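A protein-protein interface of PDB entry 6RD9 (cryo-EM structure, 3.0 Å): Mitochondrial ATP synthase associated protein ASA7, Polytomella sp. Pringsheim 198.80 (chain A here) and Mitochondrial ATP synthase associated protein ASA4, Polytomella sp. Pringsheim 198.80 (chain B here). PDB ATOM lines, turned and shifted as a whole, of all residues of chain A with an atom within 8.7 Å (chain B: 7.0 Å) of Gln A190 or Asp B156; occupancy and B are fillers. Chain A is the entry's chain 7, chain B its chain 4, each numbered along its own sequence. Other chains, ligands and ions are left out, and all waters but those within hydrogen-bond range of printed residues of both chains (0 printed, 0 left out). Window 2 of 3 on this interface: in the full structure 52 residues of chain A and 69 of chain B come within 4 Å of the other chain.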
ATOM      1  N   ASN A 184     -34.519 -10.386  -0.939  1.00  0.00           N
ATOM      2  CA  ASN A 184     -35.041 -11.740  -1.054  1.00  0.00           C
ATOM      3  C   ASN A 184     -34.018 -12.771  -0.606  1.00  0.00           C
ATOM      4  O   ASN A 184     -34.379 -13.793  -0.019  1.00  0.00           O
ATOM      5  CB  ASN A 184     -35.473 -12.024  -2.482  1.00  0.00           C
ATOM      6  CG  ASN A 184     -35.907 -13.443  -2.668  1.00  0.00           C
ATOM      7  OD1 ASN A 184     -35.311 -14.196  -3.430  1.00  0.00           O
ATOM      8  ND2 ASN A 184     -36.925 -13.834  -1.934  1.00  0.00           N
ATOM      9  N   PHE A 185     -32.741 -12.519  -0.855  1.00  0.00           N
ATOM     10  CA  PHE A 185     -31.734 -13.511  -0.516  1.00  0.00           C
ATOM     11  C   PHE A 185     -31.430 -13.513   0.966  1.00  0.00           C
ATOM     12  O   PHE A 185     -31.168 -14.573   1.540  1.00  0.00           O
ATOM     13  CB  PHE A 185     -30.461 -13.245  -1.302  1.00  0.00           C
ATOM     14  CG  PHE A 185     -29.315 -14.109  -0.910  1.00  0.00           C
ATOM     15  CD1 PHE A 185     -28.280 -13.606  -0.146  1.00  0.00           C
ATOM     16  CD2 PHE A 185     -29.251 -15.413  -1.333  1.00  0.00           C
ATOM     17  CE1 PHE A 185     -27.222 -14.394   0.200  1.00  0.00           C
ATOM     18  CE2 PHE A 185     -28.190 -16.202  -0.992  1.00  0.00           C
ATOM     19  CZ  PHE A 185     -27.179 -15.689  -0.224  1.00  0.00           C
ATOM     20  N   LEU A 186     -31.439 -12.346   1.599  1.00  0.00           N
ATOM     21  CA  LEU A 186     -31.042 -12.281   2.996  1.00  0.00           C
ATOM     22  C   LEU A 186     -32.218 -12.602   3.902  1.00  0.00           C
ATOM     23  O   LEU A 186     -32.082 -13.360   4.859  1.00  0.00           O
ATOM     24  CB  LEU A 186     -30.479 -10.904   3.315  1.00  0.00           C
ATOM     25  CG  LEU A 186     -29.566 -10.825   4.518  1.00  0.00           C
ATOM     26  CD1 LEU A 186     -28.325 -11.603   4.194  1.00  0.00           C
ATOM     27  CD2 LEU A 186     -29.224  -9.399   4.804  1.00  0.00           C
ATOM     28  N   LEU A 187     -33.394 -12.069   3.589  1.00  0.00           N
ATOM     29  CA  LEU A 187     -34.575 -12.292   4.410  1.00  0.00           C
ATOM     30  C   LEU A 187     -35.336 -13.545   4.016  1.00  0.00           C
ATOM     31  O   LEU A 187     -36.554 -13.610   4.205  1.00  0.00           O
ATOM     32  CB  LEU A 187     -35.506 -11.086   4.366  1.00  0.00           C
ATOM     33  CG  LEU A 187     -34.966  -9.678   4.580  1.00  0.00           C
ATOM     34  CD1 LEU A 187     -36.141  -8.774   4.802  1.00  0.00           C
ATOM     35  CD2 LEU A 187     -33.997  -9.587   5.726  1.00  0.00           C
ATOM     36  N   SER A 188     -34.665 -14.520   3.431  1.00  0.00           N
ATOM     37  CA  SER A 188     -35.125 -15.894   3.431  1.00  0.00           C
ATOM     38  C   SER A 188     -34.127 -16.725   4.224  1.00  0.00           C
ATOM     39  O   SER A 188     -33.069 -16.241   4.631  1.00  0.00           O
ATOM     40  CB  SER A 188     -35.295 -16.422   2.010  1.00  0.00           C
ATOM     41  OG  SER A 188     -36.094 -15.543   1.249  1.00  0.00           O
ATOM     42  N   LYS A 189     -34.477 -17.981   4.457  1.00  0.00           N
ATOM     43  CA  LYS A 189     -33.630 -18.853   5.255  1.00  0.00           C
ATOM     44  C   LYS A 189     -32.385 -19.236   4.460  1.00  0.00           C
ATOM     45  O   LYS A 189     -32.485 -19.732   3.332  1.00  0.00           O
ATOM     46  CB  LYS A 189     -34.431 -20.069   5.728  1.00  0.00           C
ATOM     47  CG  LYS A 189     -35.105 -20.892   4.641  1.00  0.00           C
ATOM     48  CD  LYS A 189     -36.061 -21.883   5.217  1.00  0.00           C
ATOM     49  CE  LYS A 189     -37.246 -21.130   5.757  1.00  0.00           C
ATOM     50  NZ  LYS A 189     -37.934 -20.390   4.673  1.00  0.00           N
ATOM     51  N   GLN A 190     -31.227 -18.930   5.050  1.00  0.00           N
ATOM     52  CA  GLN A 190     -29.851 -19.149   4.573  1.00  0.00           C
ATOM     53  C   GLN A 190     -29.599 -19.260   3.069  1.00  0.00           C
ATOM     54  O   GLN A 190     -30.078 -18.439   2.287  1.00  0.00           O
ATOM     55  CB  GLN A 190     -29.260 -20.394   5.234  1.00  0.00           C
ATOM     56  CG  GLN A 190     -29.731 -21.738   4.693  1.00  0.00           C
ATOM     57  CD  GLN A 190     -30.876 -22.358   5.477  1.00  0.00           C
ATOM     58  OE1 GLN A 190     -31.593 -21.683   6.206  1.00  0.00           O
ATOM     59  NE2 GLN A 190     -31.029 -23.668   5.345  1.00  0.00           N
ATOM     60  N   THR B 113     -21.792 -17.057  -1.673  1.00  0.00           N
ATOM     61  CA  THR B 113     -21.925 -17.355  -0.255  1.00  0.00           C
ATOM     62  C   THR B 113     -22.407 -18.776  -0.014  1.00  0.00           C
ATOM     63  O   THR B 113     -23.312 -18.994   0.795  1.00  0.00           O
ATOM     64  CB  THR B 113     -22.891 -16.384   0.406  1.00  0.00           C
ATOM     65  OG1 THR B 113     -24.118 -16.387  -0.317  1.00  0.00           O
ATOM     66  CG2 THR B 113     -22.330 -15.000   0.393  1.00  0.00           C
ATOM     67  N   SER B 116     -20.826 -19.866   3.668  1.00  0.00           N
ATOM     68  CA  SER B 116     -20.987 -18.967   4.797  1.00  0.00           C
ATOM     69  C   SER B 116     -22.161 -19.409   5.652  1.00  0.00           C
ATOM     70  O   SER B 116     -23.222 -19.756   5.126  1.00  0.00           O
ATOM     71  CB  SER B 116     -21.196 -17.535   4.313  1.00  0.00           C
ATOM     72  OG  SER B 116     -20.236 -17.191   3.331  1.00  0.00           O
ATOM     73  N   GLU B 117     -21.959 -19.406   6.967  1.00  0.00           N
ATOM     74  CA  GLU B 117     -23.050 -19.634   7.904  1.00  0.00           C
ATOM     75  C   GLU B 117     -23.206 -18.483   8.885  1.00  0.00           C
ATOM     76  O   GLU B 117     -24.098 -18.536   9.741  1.00  0.00           O
ATOM     77  CB  GLU B 117     -22.860 -20.954   8.661  1.00  0.00           C
ATOM     78  CG  GLU B 117     -21.551 -21.065   9.419  1.00  0.00           C
ATOM     79  CD  GLU B 117     -20.477 -21.776   8.611  1.00  0.00           C
ATOM     80  OE1 GLU B 117     -20.687 -21.999   7.401  1.00  0.00           O
ATOM     81  OE2 GLU B 117     -19.418 -22.105   9.180  1.00  0.00           O
ATOM     82  N   THR B 118     -22.389 -17.446   8.780  1.00  0.00           N
ATOM     83  CA  THR B 118     -22.563 -16.227   9.547  1.00  0.00           C
ATOM     84  C   THR B 118     -22.928 -15.075   8.625  1.00  0.00           C
ATOM     85  O   THR B 118     -22.526 -15.036   7.460  1.00  0.00           O
ATOM     86  CB  THR B 118     -21.302 -15.887  10.333  1.00  0.00           C
ATOM     87  OG1 THR B 118     -21.417 -14.558  10.850  1.00  0.00           O
ATOM     88  CG2 THR B 118     -20.076 -16.005   9.456  1.00  0.00           C
ATOM     89  N   VAL B 119     -23.689 -14.128   9.167  1.00  0.00           N
ATOM     90  CA  VAL B 119     -24.221 -13.039   8.361  1.00  0.00           C
ATOM     91  C   VAL B 119     -23.140 -12.017   8.038  1.00  0.00           C
ATOM     92  O   VAL B 119     -23.130 -11.448   6.944  1.00  0.00           O
ATOM     93  CB  VAL B 119     -25.426 -12.431   9.097  1.00  0.00           C
ATOM     94  CG1 VAL B 119     -25.931 -11.194   8.427  1.00  0.00           C
ATOM     95  CG2 VAL B 119     -26.534 -13.442   9.144  1.00  0.00           C
ATOM     96  N   VAL B 153     -24.290 -13.267  14.469  1.00  0.00           N
ATOM     97  CA  VAL B 153     -25.599 -13.632  13.939  1.00  0.00           C
ATOM     98  C   VAL B 153     -25.393 -14.663  12.844  1.00  0.00           C
ATOM     99  O   VAL B 153     -24.609 -14.449  11.915  1.00  0.00           O
ATOM    100  CB  VAL B 153     -26.357 -12.411  13.413  1.00  0.00           C
ATOM    101  CG1 VAL B 153     -27.711 -12.837  12.900  1.00  0.00           C
ATOM    102  CG2 VAL B 153     -26.529 -11.395  14.496  1.00  0.00           C
ATOM    103  N   LEU B 154     -26.065 -15.796  12.973  1.00  0.00           N
ATOM    104  CA  LEU B 154     -25.852 -16.914  12.077  1.00  0.00           C
ATOM    105  C   LEU B 154     -26.737 -16.806  10.848  1.00  0.00           C
ATOM    106  O   LEU B 154     -27.830 -16.236  10.893  1.00  0.00           O
ATOM    107  CB  LEU B 154     -26.122 -18.235  12.793  1.00  0.00           C
ATOM    108  CG  LEU B 154     -25.143 -18.614  13.897  1.00  0.00           C
ATOM    109  CD1 LEU B 154     -25.412 -20.035  14.335  1.00  0.00           C
ATOM    110  CD2 LEU B 154     -23.697 -18.442  13.453  1.00  0.00           C
ATOM    111  N   PHE B 155     -26.247 -17.367   9.746  1.00  0.00           N
ATOM    112  CA  PHE B 155     -27.029 -17.509   8.523  1.00  0.00           C
ATOM    113  C   PHE B 155     -27.748 -18.858   8.587  1.00  0.00           C
ATOM    114  O   PHE B 155     -27.388 -19.833   7.928  1.00  0.00           O
ATOM    115  CB  PHE B 155     -26.114 -17.388   7.312  1.00  0.00           C
ATOM    116  CG  PHE B 155     -26.801 -16.934   6.064  1.00  0.00           C
ATOM    117  CD1 PHE B 155     -27.733 -15.915   6.103  1.00  0.00           C
ATOM    118  CD2 PHE B 155     -26.478 -17.500   4.843  1.00  0.00           C
ATOM    119  CE1 PHE B 155     -28.353 -15.492   4.954  1.00  0.00           C
ATOM    120  CE2 PHE B 155     -27.083 -17.070   3.691  1.00  0.00           C
ATOM    121  CZ  PHE B 155     -28.032 -16.074   3.751  1.00  0.00           C
ATOM    122  N   ASP B 156     -28.764 -18.908   9.440  1.00  0.00           N
ATOM    123  CA  ASP B 156     -29.519 -20.132   9.677  1.00  0.00           C
ATOM    124  C   ASP B 156     -31.008 -19.976   9.432  1.00  0.00           C
ATOM    125  O   ASP B 156     -31.646 -20.902   8.935  1.00  0.00           O
ATOM    126  CB  ASP B 156     -29.282 -20.626  11.115  1.00  0.00           C
ATOM    127  CG  ASP B 156     -30.290 -21.682  11.553  1.00  0.00           C
ATOM    128  OD1 ASP B 156     -30.358 -22.750  10.910  1.00  0.00           O
ATOM    129  OD2 ASP B 156     -31.020 -21.447  12.538  1.00  0.00           O
ATOM    130  N   GLY B 157     -31.584 -18.843   9.765  1.00  0.00           N
ATOM    131  CA  GLY B 157     -33.003 -18.637   9.509  1.00  0.00           C
ATOM    132  C   GLY B 157     -33.912 -19.101  10.611  1.00  0.00           C
ATOM    133  O   GLY B 157     -34.827 -18.380  11.007  1.00  0.00           O
ATOM    134  N   LYS B 158     -33.675 -20.309  11.120  1.00  0.00           N
ATOM    135  CA  LYS B 158     -34.401 -20.843  12.261  1.00  0.00           C
ATOM    136  C   LYS B 158     -33.844 -20.357  13.587  1.00  0.00           C
ATOM    137  O   LYS B 158     -34.534 -20.458  14.604  1.00  0.00           O
ATOM    138  CB  LYS B 158     -34.372 -22.370  12.237  1.00  0.00           C
ATOM    139  CG  LYS B 158     -35.024 -22.984  11.016  1.00  0.00           C
ATOM    140  CD  LYS B 158     -35.015 -24.497  11.111  1.00  0.00           C
ATOM    141  CE  LYS B 158     -33.597 -25.050  11.015  1.00  0.00           C
ATOM    142  NZ  LYS B 158     -32.982 -24.804   9.688  1.00  0.00           N
ATOM    143  N   THR B 159     -32.621 -19.839  13.593  1.00  0.00           N
ATOM    144  CA  THR B 159     -32.083 -19.168  14.764  1.00  0.00           C
ATOM    145  C   THR B 159     -32.886 -17.905  15.039  1.00  0.00           C
ATOM    146  O   THR B 159     -33.144 -17.115  14.129  1.00  0.00           O
ATOM    147  CB  THR B 159     -30.616 -18.828  14.530  1.00  0.00           C
ATOM    148  OG1 THR B 159     -29.882 -20.038  14.334  1.00  0.00           O
ATOM    149  CG2 THR B 159     -30.034 -18.105  15.703  1.00  0.00           C
ATOM    150  N   GLU B 160     -33.316 -17.730  16.287  1.00  0.00           N
ATOM    151  CA  GLU B 160     -34.046 -16.523  16.643  1.00  0.00           C
ATOM    152  C   GLU B 160     -33.128 -15.306  16.657  1.00  0.00           C
ATOM    153  O   GLU B 160     -33.602 -14.182  16.466  1.00  0.00           O
ATOM    154  CB  GLU B 160     -34.750 -16.743  17.993  1.00  0.00           C
ATOM    155  CG  GLU B 160     -35.660 -15.615  18.507  1.00  0.00           C
ATOM    156  CD  GLU B 160     -34.933 -14.528  19.279  1.00  0.00           C
ATOM    157  OE1 GLU B 160     -35.538 -13.460  19.497  1.00  0.00           O
ATOM    158  OE2 GLU B 160     -33.773 -14.742  19.683  1.00  0.00           O
ATOM    159  N   PHE B 162     -31.158 -14.570  14.331  1.00  0.00           N
ATOM    160  CA  PHE B 162     -31.324 -14.046  12.989  1.00  0.00           C
ATOM    161  C   PHE B 162     -32.705 -13.450  12.773  1.00  0.00           C
ATOM    162  O   PHE B 162     -32.846 -12.526  11.970  1.00  0.00           O
ATOM    163  CB  PHE B 162     -31.073 -15.166  11.977  1.00  0.00           C
ATOM    164  CG  PHE B 162     -31.226 -14.748  10.545  1.00  0.00           C
ATOM    165  CD1 PHE B 162     -30.231 -14.026   9.913  1.00  0.00           C
ATOM    166  CD2 PHE B 162     -32.364 -15.081   9.829  1.00  0.00           C
ATOM    167  CE1 PHE B 162     -30.370 -13.644   8.601  1.00  0.00           C
ATOM    168  CE2 PHE B 162     -32.504 -14.700   8.526  1.00  0.00           C
ATOM    169  CZ  PHE B 162     -31.505 -13.985   7.914  1.00  0.00           C
ATOM    170  N   LYS B 163     -33.718 -13.947  13.489  1.00  0.00           N
ATOM    171  CA  LYS B 163     -35.104 -13.578  13.205  1.00  0.00           C
ATOM    172  C   LYS B 163     -35.396 -12.124  13.551  1.00  0.00           C
ATOM    173  O   LYS B 163     -36.177 -11.463  12.860  1.00  0.00           O
ATOM    174  CB  LYS B 163     -36.057 -14.483  13.974  1.00  0.00           C
ATOM    175  CG  LYS B 163     -36.334 -15.794  13.311  1.00  0.00           C
ATOM    176  CD  LYS B 163     -37.573 -16.419  13.905  1.00  0.00           C
ATOM    177  CE  LYS B 163     -37.745 -17.829  13.403  1.00  0.00           C
ATOM    178  NZ  LYS B 163     -36.567 -18.660  13.764  1.00  0.00           N
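The backbone carbonyl oxygen (O) of Asp B156 sits close to the side-chain amide oxygen (OE1) of Gln A190 (2.8 Å).
The side-chain carboxylate of Asp B156 is in hydrogen-bond range of the backbone NH of Thr B159, at 2.5 Å. The side-chain amino group of Lys B158 lies within salt-bridge range of the side-chain carboxylate of Asp B156, 3.5 Å away. The backbone carbonyl oxygen (O) of Glu B117 lies within hydrogen-bond range of the backbone NH (N) of Phe B155 (2.4 Å).
Among the printed residues, pairs that only touch across the chains: Phe A185 with Thr B113 (3.1 Å), Leu A186 with Phe B155 (3.96 Å), Leu A186 with Phe B162 (3.2 Å) and Gln A190 with Phe B155 (3.3 Å).
Gln A190 touches two residues of chain B. Printed residues of chain A within 4 Å of Phe B155: Leu A186 and Gln A190. Asp B156 touches one residue of chain A. No residue of chain A comes within 4 Å of Gly B157. Printed residues of chain A within 4 Å of Phe B162: Leu A186. The nearest residue of chain A that does not touch Asp B156 is Lys A189 (4.3 Å).
Hydrophobic or aromatic side chains of chain B that line the printed part of chain A: Phe B155 and Phe B162. Along chain B the printed residues that touch a printed residue of chain A span positions 113 to 162. Of the 7 printed residues of chain A, 3 touch a printed residue of chain B. Among the printed residues, 5 pairs touch across the chains.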
